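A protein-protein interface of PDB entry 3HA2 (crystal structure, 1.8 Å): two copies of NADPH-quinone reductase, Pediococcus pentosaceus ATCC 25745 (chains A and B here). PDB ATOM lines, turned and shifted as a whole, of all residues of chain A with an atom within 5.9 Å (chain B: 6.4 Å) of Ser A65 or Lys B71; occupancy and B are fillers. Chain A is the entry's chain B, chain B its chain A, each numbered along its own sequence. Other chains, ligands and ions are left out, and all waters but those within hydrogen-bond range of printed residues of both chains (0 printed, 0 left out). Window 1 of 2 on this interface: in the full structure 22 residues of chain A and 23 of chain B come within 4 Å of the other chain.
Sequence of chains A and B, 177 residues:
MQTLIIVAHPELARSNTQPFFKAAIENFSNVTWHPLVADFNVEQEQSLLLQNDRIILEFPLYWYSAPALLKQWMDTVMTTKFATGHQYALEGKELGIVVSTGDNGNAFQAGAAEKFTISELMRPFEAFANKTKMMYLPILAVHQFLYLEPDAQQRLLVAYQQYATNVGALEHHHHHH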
ATOM      1  N   PHE A  59      23.252  -5.318  -1.691  1.00  0.00           N
ATOM      2  CA  PHE A  59      22.544  -5.831  -0.525  1.00  0.00           C
ATOM      3  C   PHE A  59      23.377  -5.834   0.766  1.00  0.00           C
ATOM      4  O   PHE A  59      24.609  -5.873   0.720  1.00  0.00           O
ATOM      5  CB  PHE A  59      22.032  -7.253  -0.799  1.00  0.00           C
ATOM      6  CG  PHE A  59      23.129  -8.249  -1.172  1.00  0.00           C
ATOM      7  CD1 PHE A  59      23.497  -8.431  -2.501  1.00  0.00           C
ATOM      8  CD2 PHE A  59      23.791  -8.985  -0.191  1.00  0.00           C
ATOM      9  CE1 PHE A  59      24.498  -9.348  -2.863  1.00  0.00           C
ATOM     10  CE2 PHE A  59      24.784  -9.894  -0.537  1.00  0.00           C
ATOM     11  CZ  PHE A  59      25.140 -10.070  -1.888  1.00  0.00           C
ATOM     12  N   PRO A  60      22.693  -5.828   1.922  1.00  0.00           N
ATOM     13  CA  PRO A  60      23.376  -6.050   3.199  1.00  0.00           C
ATOM     14  C   PRO A  60      23.643  -7.532   3.430  1.00  0.00           C
ATOM     15  O   PRO A  60      22.861  -8.397   3.010  1.00  0.00           O
ATOM     16  CB  PRO A  60      22.375  -5.513   4.228  1.00  0.00           C
ATOM     17  CG  PRO A  60      21.020  -5.779   3.583  1.00  0.00           C
ATOM     18  CD  PRO A  60      21.243  -5.611   2.091  1.00  0.00           C
ATOM     19  N   LEU A  61      24.746  -7.829   4.102  1.00  0.00           N
ATOM     20  CA  LEU A  61      25.068  -9.202   4.471  1.00  0.00           C
ATOM     21  C   LEU A  61      24.225  -9.605   5.680  1.00  0.00           C
ATOM     22  O   LEU A  61      24.371  -9.040   6.760  1.00  0.00           O
ATOM     23  CB  LEU A  61      26.557  -9.301   4.836  1.00  0.00           C
ATOM     24  CG  LEU A  61      27.124 -10.721   4.869  1.00  0.00           C
ATOM     25  CD1 LEU A  61      27.216 -11.311   3.462  1.00  0.00           C
ATOM     26  CD2 LEU A  61      28.494 -10.701   5.557  1.00  0.00           C
ATOM     27  N   TYR A  62      23.329 -10.571   5.486  1.00  0.00           N
ATOM     28  CA  TYR A  62      22.455 -11.052   6.540  1.00  0.00           C
ATOM     29  C   TYR A  62      22.844 -12.504   6.811  1.00  0.00           C
ATOM     30  O   TYR A  62      22.628 -13.349   5.957  1.00  0.00           O
ATOM     31  CB  TYR A  62      21.019 -11.011   6.032  1.00  0.00           C
ATOM     32  CG  TYR A  62      20.301  -9.690   6.185  1.00  0.00           C
ATOM     33  CD1 TYR A  62      20.978  -8.517   6.550  1.00  0.00           C
ATOM     34  CD2 TYR A  62      18.929  -9.615   5.953  1.00  0.00           C
ATOM     35  CE1 TYR A  62      20.289  -7.306   6.702  1.00  0.00           C
ATOM     36  CE2 TYR A  62      18.239  -8.413   6.100  1.00  0.00           C
ATOM     37  CZ  TYR A  62      18.928  -7.269   6.462  1.00  0.00           C
ATOM     38  OH  TYR A  62      18.233  -6.093   6.617  1.00  0.00           O
ATOM     39  N   TRP A  63      23.407 -12.790   7.984  1.00  0.00           N
ATOM     40  CA  TRP A  63      23.947 -14.127   8.304  1.00  0.00           C
ATOM     41  C   TRP A  63      24.775 -14.688   7.131  1.00  0.00           C
ATOM     42  O   TRP A  63      24.535 -15.801   6.647  1.00  0.00           O
ATOM     43  CB  TRP A  63      22.839 -15.124   8.736  1.00  0.00           C
ATOM     44  CG  TRP A  63      22.197 -14.768  10.069  1.00  0.00           C
ATOM     45  CD1 TRP A  63      20.875 -14.478  10.286  1.00  0.00           C
ATOM     46  CD2 TRP A  63      22.850 -14.629  11.338  1.00  0.00           C
ATOM     47  NE1 TRP A  63      20.664 -14.185  11.611  1.00  0.00           N
ATOM     48  CE2 TRP A  63      21.855 -14.279  12.285  1.00  0.00           C
ATOM     49  CE3 TRP A  63      24.178 -14.785  11.776  1.00  0.00           C
ATOM     50  CZ2 TRP A  63      22.147 -14.054  13.638  1.00  0.00           C
ATOM     51  CZ3 TRP A  63      24.462 -14.577  13.119  1.00  0.00           C
ATOM     52  CH2 TRP A  63      23.449 -14.221  14.039  1.00  0.00           C
ATOM     53  N   TYR A  64      25.735 -13.887   6.669  1.00  0.00           N
ATOM     54  CA  TYR A  64      26.773 -14.340   5.740  1.00  0.00           C
ATOM     55  C   TYR A  64      26.242 -14.621   4.336  1.00  0.00           C
ATOM     56  O   TYR A  64      26.922 -15.234   3.518  1.00  0.00           O
ATOM     57  CB  TYR A  64      27.526 -15.554   6.321  1.00  0.00           C
ATOM     58  CG  TYR A  64      28.023 -15.281   7.727  1.00  0.00           C
ATOM     59  CD1 TYR A  64      29.159 -14.497   7.950  1.00  0.00           C
ATOM     60  CD2 TYR A  64      27.325 -15.760   8.843  1.00  0.00           C
ATOM     61  CE1 TYR A  64      29.596 -14.224   9.253  1.00  0.00           C
ATOM     62  CE2 TYR A  64      27.734 -15.466  10.148  1.00  0.00           C
ATOM     63  CZ  TYR A  64      28.875 -14.711  10.346  1.00  0.00           C
ATOM     64  OH  TYR A  64      29.293 -14.435  11.627  1.00  0.00           O
ATOM     65  N   SER A  65      25.033 -14.150   4.062  1.00  0.00           N
ATOM     66  CA  SER A  65      24.443 -14.284   2.738  1.00  0.00           C
ATOM     67  C   SER A  65      23.523 -13.118   2.372  1.00  0.00           C
ATOM     68  O   SER A  65      23.267 -12.231   3.188  1.00  0.00           O
ATOM     69  CB  SER A  65      23.713 -15.633   2.632  1.00  0.00           C
ATOM     70  OG  SER A  65      22.828 -15.804   3.722  1.00  0.00           O
ATOM     71  N   ALA A  66      23.047 -13.099   1.129  1.00  0.00           N
ATOM     72  CA  ALA A  66      22.083 -12.076   0.716  1.00  0.00           C
ATOM     73  C   ALA A  66      20.762 -12.284   1.454  1.00  0.00           C
ATOM     74  O   ALA A  66      20.446 -13.416   1.836  1.00  0.00           O
ATOM     75  CB  ALA A  66      21.847 -12.153  -0.804  1.00  0.00           C
ATOM     76  N   PRO A  67      20.000 -11.198   1.652  1.00  0.00           N
ATOM     77  CA  PRO A  67      18.656 -11.228   2.238  1.00  0.00           C
ATOM     78  C   PRO A  67      17.697 -12.082   1.428  1.00  0.00           C
ATOM     79  O   PRO A  67      17.905 -12.300   0.224  1.00  0.00           O
ATOM     80  CB  PRO A  67      18.197  -9.767   2.167  1.00  0.00           C
ATOM     81  CG  PRO A  67      19.434  -8.982   1.997  1.00  0.00           C
ATOM     82  CD  PRO A  67      20.406  -9.829   1.287  1.00  0.00           C
ATOM     83  N   ALA A  68      16.649 -12.562   2.097  1.00  0.00           N
ATOM     84  CA  ALA A  68      15.638 -13.403   1.472  1.00  0.00           C
ATOM     85  C   ALA A  68      15.038 -12.782   0.207  1.00  0.00           C
ATOM     86  O   ALA A  68      14.732 -13.514  -0.728  1.00  0.00           O
ATOM     87  CB  ALA A  68      14.499 -13.689   2.467  1.00  0.00           C
ATOM     88  N   LYS A  71      17.219 -13.561  -2.632  1.00  0.00           N
ATOM     89  CA  LYS A  71      17.147 -14.994  -2.913  1.00  0.00           C
ATOM     90  C   LYS A  71      15.872 -15.323  -3.683  1.00  0.00           C
ATOM     91  O   LYS A  71      15.888 -16.135  -4.622  1.00  0.00           O
ATOM     92  CB  LYS A  71      17.289 -15.835  -1.630  1.00  0.00           C
ATOM     93  CG  LYS A  71      17.615 -17.321  -1.919  1.00  0.00           C
ATOM     94  CD  LYS A  71      18.927 -17.436  -2.725  1.00  0.00           C
ATOM     95  CE  LYS A  71      18.834 -18.440  -3.850  1.00  0.00           C
ATOM     96  NZ  LYS A  71      18.272 -19.781  -3.463  1.00  0.00           N
ATOM     97  N   LEU A 121      32.472 -16.423   0.937  1.00  0.00           N
ATOM     98  CA  LEU A 121      31.057 -16.357   1.311  1.00  0.00           C
ATOM     99  C   LEU A 121      30.175 -16.078   0.103  1.00  0.00           C
ATOM    100  O   LEU A 121      29.022 -16.515   0.075  1.00  0.00           O
ATOM    101  CB  LEU A 121      30.814 -15.296   2.402  1.00  0.00           C
ATOM    102  CG  LEU A 121      31.530 -15.618   3.712  1.00  0.00           C
ATOM    103  CD1 LEU A 121      31.475 -14.399   4.644  1.00  0.00           C
ATOM    104  CD2 LEU A 121      30.953 -16.877   4.376  1.00  0.00           C
ATOM    105  N   MET A 122      30.724 -15.380  -0.892  1.00  0.00           N
ATOM    106  CA  MET A 122      29.940 -14.994  -2.084  1.00  0.00           C
ATOM    107  C   MET A 122      29.953 -16.085  -3.166  1.00  0.00           C
ATOM    108  O   MET A 122      29.435 -15.890  -4.281  1.00  0.00           O
ATOM    109  CB  MET A 122      30.432 -13.655  -2.648  1.00  0.00           C
ATOM    110  CG  MET A 122      30.217 -12.427  -1.732  1.00  0.00           C
ATOM    111  SD  MET A 122      28.309 -12.076  -1.296  1.00  0.00           S
ATOM    112  CE  MET A 122      28.225 -12.969   0.445  1.00  0.00           C
ATOM    113  N   LEU B  36       8.535 -25.796   7.257  1.00  0.00           N
ATOM    114  CA  LEU B  36       8.580 -24.354   7.286  1.00  0.00           C
ATOM    115  C   LEU B  36       7.444 -23.814   6.422  1.00  0.00           C
ATOM    116  O   LEU B  36       7.364 -24.091   5.212  1.00  0.00           O
ATOM    117  CB  LEU B  36       9.959 -23.893   6.796  1.00  0.00           C
ATOM    118  CG  LEU B  36      10.342 -22.426   6.739  1.00  0.00           C
ATOM    119  CD1 LEU B  36      10.036 -21.724   8.054  1.00  0.00           C
ATOM    120  CD2 LEU B  36      11.839 -22.329   6.405  1.00  0.00           C
ATOM    121  N   ALA B  66      20.322 -22.038  -0.185  1.00  0.00           N
ATOM    122  CA  ALA B  66      19.005 -22.366   0.343  1.00  0.00           C
ATOM    123  C   ALA B  66      17.881 -21.570  -0.338  1.00  0.00           C
ATOM    124  O   ALA B  66      18.119 -20.450  -0.787  1.00  0.00           O
ATOM    125  CB  ALA B  66      18.997 -22.109   1.852  1.00  0.00           C
ATOM    126  N   PRO B  67      16.661 -22.139  -0.404  1.00  0.00           N
ATOM    127  CA  PRO B  67      15.476 -21.426  -0.895  1.00  0.00           C
ATOM    128  C   PRO B  67      15.203 -20.174  -0.055  1.00  0.00           C
ATOM    129  O   PRO B  67      15.597 -20.078   1.117  1.00  0.00           O
ATOM    130  CB  PRO B  67      14.326 -22.429  -0.691  1.00  0.00           C
ATOM    131  CG  PRO B  67      14.993 -23.748  -0.574  1.00  0.00           C
ATOM    132  CD  PRO B  67      16.346 -23.524  -0.016  1.00  0.00           C
ATOM    133  N   ALA B  68      14.517 -19.222  -0.662  1.00  0.00           N
ATOM    134  CA  ALA B  68      14.255 -17.944  -0.014  1.00  0.00           C
ATOM    135  C   ALA B  68      13.489 -18.069   1.318  1.00  0.00           C
ATOM    136  O   ALA B  68      13.738 -17.300   2.241  1.00  0.00           O
ATOM    137  CB  ALA B  68      13.508 -17.042  -0.968  1.00  0.00           C
ATOM    138  N   LEU B  69      12.547 -19.008   1.414  1.00  0.00           N
ATOM    139  CA  LEU B  69      11.790 -19.144   2.675  1.00  0.00           C
ATOM    140  C   LEU B  69      12.715 -19.535   3.829  1.00  0.00           C
ATOM    141  O   LEU B  69      12.540 -19.040   4.937  1.00  0.00           O
ATOM    142  CB  LEU B  69      10.613 -20.132   2.582  1.00  0.00           C
ATOM    143  CG  LEU B  69       9.659 -20.061   3.815  1.00  0.00           C
ATOM    144  CD1 LEU B  69       9.117 -18.652   4.090  1.00  0.00           C
ATOM    145  CD2 LEU B  69       8.485 -21.019   3.729  1.00  0.00           C
ATOM    146  N   LEU B  70      13.708 -20.386   3.578  1.00  0.00           N
ATOM    147  CA  LEU B  70      14.667 -20.696   4.650  1.00  0.00           C
ATOM    148  C   LEU B  70      15.520 -19.473   5.014  1.00  0.00           C
ATOM    149  O   LEU B  70      15.792 -19.229   6.188  1.00  0.00           O
ATOM    150  CB  LEU B  70      15.554 -21.905   4.326  1.00  0.00           C
ATOM    151  CG  LEU B  70      16.546 -22.296   5.444  1.00  0.00           C
ATOM    152  CD1 LEU B  70      15.832 -22.656   6.763  1.00  0.00           C
ATOM    153  CD2 LEU B  70      17.447 -23.434   5.012  1.00  0.00           C
ATOM    154  N   LYS B  71      15.916 -18.692   4.005  1.00  0.00           N
ATOM    155  CA  LYS B  71      16.712 -17.504   4.265  1.00  0.00           C
ATOM    156  C   LYS B  71      15.875 -16.508   5.070  1.00  0.00           C
ATOM    157  O   LYS B  71      16.385 -15.861   5.982  1.00  0.00           O
ATOM    158  CB  LYS B  71      17.173 -16.858   2.956  1.00  0.00           C
ATOM    159  CG  LYS B  71      18.152 -15.722   3.165  1.00  0.00           C
ATOM    160  CD  LYS B  71      19.477 -16.280   3.710  1.00  0.00           C
ATOM    161  CE  LYS B  71      19.996 -15.486   4.897  1.00  0.00           C
ATOM    162  NZ  LYS B  71      20.253 -14.038   4.624  1.00  0.00           N
ATOM    163  N   GLN B  72      14.582 -16.405   4.745  1.00  0.00           N
ATOM    164  CA  GLN B  72      13.688 -15.540   5.521  1.00  0.00           C
ATOM    165  C   GLN B  72      13.608 -15.975   6.989  1.00  0.00           C
ATOM    166  O   GLN B  72      13.613 -15.142   7.887  1.00  0.00           O
ATOM    167  CB  GLN B  72      12.288 -15.470   4.915  1.00  0.00           C
ATOM    168  CG  GLN B  72      11.389 -14.380   5.548  1.00  0.00           C
ATOM    169  CD  GLN B  72      11.924 -12.979   5.281  1.00  0.00           C
ATOM    170  OE1 GLN B  72      12.702 -12.434   6.061  1.00  0.00           O
ATOM    171  NE2 GLN B  72      11.561 -12.422   4.134  1.00  0.00           N
ATOM    172  N   TRP B  73      13.541 -17.285   7.220  1.00  0.00           N
ATOM    173  CA  TRP B  73      13.501 -17.830   8.588  1.00  0.00           C
ATOM    174  C   TRP B  73      14.794 -17.494   9.319  1.00  0.00           C
ATOM    175  O   TRP B  73      14.768 -17.072  10.475  1.00  0.00           O
ATOM    176  CB  TRP B  73      13.276 -19.340   8.477  1.00  0.00           C
ATOM    177  CG  TRP B  73      13.178 -20.155   9.740  1.00  0.00           C
ATOM    178  CD1 TRP B  73      12.049 -20.458  10.449  1.00  0.00           C
ATOM    179  CD2 TRP B  73      14.242 -20.877  10.349  1.00  0.00           C
ATOM    180  NE1 TRP B  73      12.361 -21.296  11.501  1.00  0.00           N
ATOM    181  CE2 TRP B  73      13.706 -21.551  11.471  1.00  0.00           C
ATOM    182  CE3 TRP B  73      15.619 -20.968  10.093  1.00  0.00           C
ATOM    183  CZ2 TRP B  73      14.491 -22.347  12.316  1.00  0.00           C
ATOM    184  CZ3 TRP B  73      16.405 -21.787  10.932  1.00  0.00           C
ATOM    185  CH2 TRP B  73      15.827 -22.451  12.034  1.00  0.00           C
ATOM    186  N   MET B  74      15.926 -17.634   8.633  1.00  0.00           N
ATOM    187  CA  MET B  74      17.218 -17.280   9.217  1.00  0.00           C
ATOM    188  C   MET B  74      17.234 -15.794   9.598  1.00  0.00           C
ATOM    189  O   MET B  74      17.629 -15.441  10.702  1.00  0.00           O
ATOM    190  CB  MET B  74      18.369 -17.578   8.238  1.00  0.00           C
ATOM    191  CG  MET B  74      18.550 -19.044   7.907  1.00  0.00           C
ATOM    192  SD  MET B  74      19.412 -19.968   9.405  1.00  0.00           S
ATOM    193  CE  MET B  74      21.083 -18.961   9.473  1.00  0.00           C
ATOM    194  N   ASP B  75      16.777 -14.939   8.674  1.00  0.00           N
ATOM    195  CA  ASP B  75      16.818 -13.474   8.841  1.00  0.00           C
ATOM    196  C   ASP B  75      15.926 -12.989   9.992  1.00  0.00           C
ATOM    197  O   ASP B  75      16.218 -11.970  10.628  1.00  0.00           O
ATOM    198  CB  ASP B  75      16.375 -12.771   7.538  1.00  0.00           C
ATOM    199  CG  ASP B  75      17.380 -12.915   6.377  1.00  0.00           C
ATOM    200  OD1 ASP B  75      18.503 -13.403   6.590  1.00  0.00           O
ATOM    201  OD2 ASP B  75      17.020 -12.520   5.240  1.00  0.00           O
ATOM    202  N   THR B  76      14.831 -13.701  10.245  1.00  0.00           N
ATOM    203  CA  THR B  76      13.779 -13.215  11.137  1.00  0.00           C
ATOM    204  C   THR B  76      13.758 -13.944  12.490  1.00  0.00           C
ATOM    205  O   THR B  76      13.544 -13.329  13.532  1.00  0.00           O
ATOM    206  CB  THR B  76      12.394 -13.314  10.435  1.00  0.00           C
ATOM    207  OG1 THR B  76      12.460 -12.682   9.141  1.00  0.00           O
ATOM    208  CG2 THR B  76      11.345 -12.603  11.227  1.00  0.00           C
ATOM    209  N   PRO B 124      28.157 -20.214   4.235  1.00  0.00           N
ATOM    210  CA  PRO B 124      27.396 -19.319   5.125  1.00  0.00           C
ATOM    211  C   PRO B 124      26.785 -20.006   6.340  1.00  0.00           C
ATOM    212  O   PRO B 124      26.669 -19.374   7.386  1.00  0.00           O
ATOM    213  CB  PRO B 124      26.295 -18.748   4.217  1.00  0.00           C
ATOM    214  CG  PRO B 124      26.816 -18.903   2.838  1.00  0.00           C
ATOM    215  CD  PRO B 124      27.658 -20.154   2.849  1.00  0.00           C
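The side-chain amino group (NZ) of Lys A71 lies within hydrogen-bond range of the backbone carbonyl oxygen (O) of Ala B66, at 2.8 Å.
The side-chain amino group of Lys B71 sits at hydrogen-bond distance from the backbone carbonyl oxygen of Tyr A62, at 2.8 Å.
NZ of Lys B71 sits close to OG of Ser A65 (3.3 Å).
NZ of Lys B71 lies within hydrogen-bond range of O of Ala A66, at 2.9 Å.
NE1 of Trp A63 is in hydrogen-bond range of O of Met B74, 3.4 Å away.
OD2 of Asp B75 lies within hydrogen-bond range of N of Ala A68 (3.2 Å).
The side-chain carboxylate of Asp B75 is in salt-bridge range of the side-chain amino group of Lys B71 (2.7 Å).
The backbone carbonyl oxygen (O) of Gln B72 sits at hydrogen-bond distance from the side-chain hydroxyl (OG1) of Thr B76 (3.0 Å).
The backbone carbonyl oxygen of Tyr A62 lies within hydrogen-bond range of the side-chain hydroxyl of Ser A65 (3.3 Å).
The side-chain hydroxyl of Ser A65 lies within hydrogen-bond range of the backbone carbonyl oxygen of Trp A63.
Tyr A62 touches Asp B75.
O of Tyr A64 touches CB of Pro B124 (3.6 Å).
Asp B75 touches Pro A67.
CB of Ala A68 touches O of Ala B68 (3.7 Å).
Ala A68 touches Lys B71 (N to CG, 3.7 Å).
Gln B72 touches Ala A68.
Lys A71 touches Ala B68 (CG to N, 3.8 Å).
Ser A65 touches just one residue of chain B: Lys B71 (3.1 Å).
Printed residues of chain B within 4 Å of Pro A67: Asp B75.
Printed residues of chain A within 4 Å of Lys B71: Tyr A62 (2.8 Å), Ser A65 (3.1 Å), Ala A66 (2.9 Å) and Ala A68 (3.7 Å).
Printed residues of chain A within 4 Å of Gln B72: Ala A68.
Thr B76 touches none of the printed residues of chain A.
Printed residues of chain A within 4 Å of Pro B124: Tyr A64 (3.6 Å).
The nearest printed residue of chain B that does not touch Tyr A62 is Met B74 (6.4 Å).
Of the 13 printed residues of chain B, 7 touch a printed residue of chain A.
Printed residues of chain B that touch a printed residue of chain A: Ala B66, Ala B68, Lys B71, Gln B72, Met B74, Asp B75 and Pro B124.
Hydrophobic or aromatic side chains of chain B within 4 Å of the printed part of chain A: Ala B68 and Pro B124.
Hydrophobic or aromatic side chains of chain A within 4 Å of the printed part of chain B: Tyr A62, Trp A63, Tyr A64 and Ala A68.
Among the printed residues, 13 pairs touch across the chains.
Ala A66 touches Lys B71, and with the chains exchanged Lys A71 touches Ala B66.
Ala B68 touches its own counterpart, Ala A68.
Ala A68 touches Lys B71, and with the chains exchanged Lys A71 touches Ala B68.
Positions printed for both chains: 66, 67, 68 and 71.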
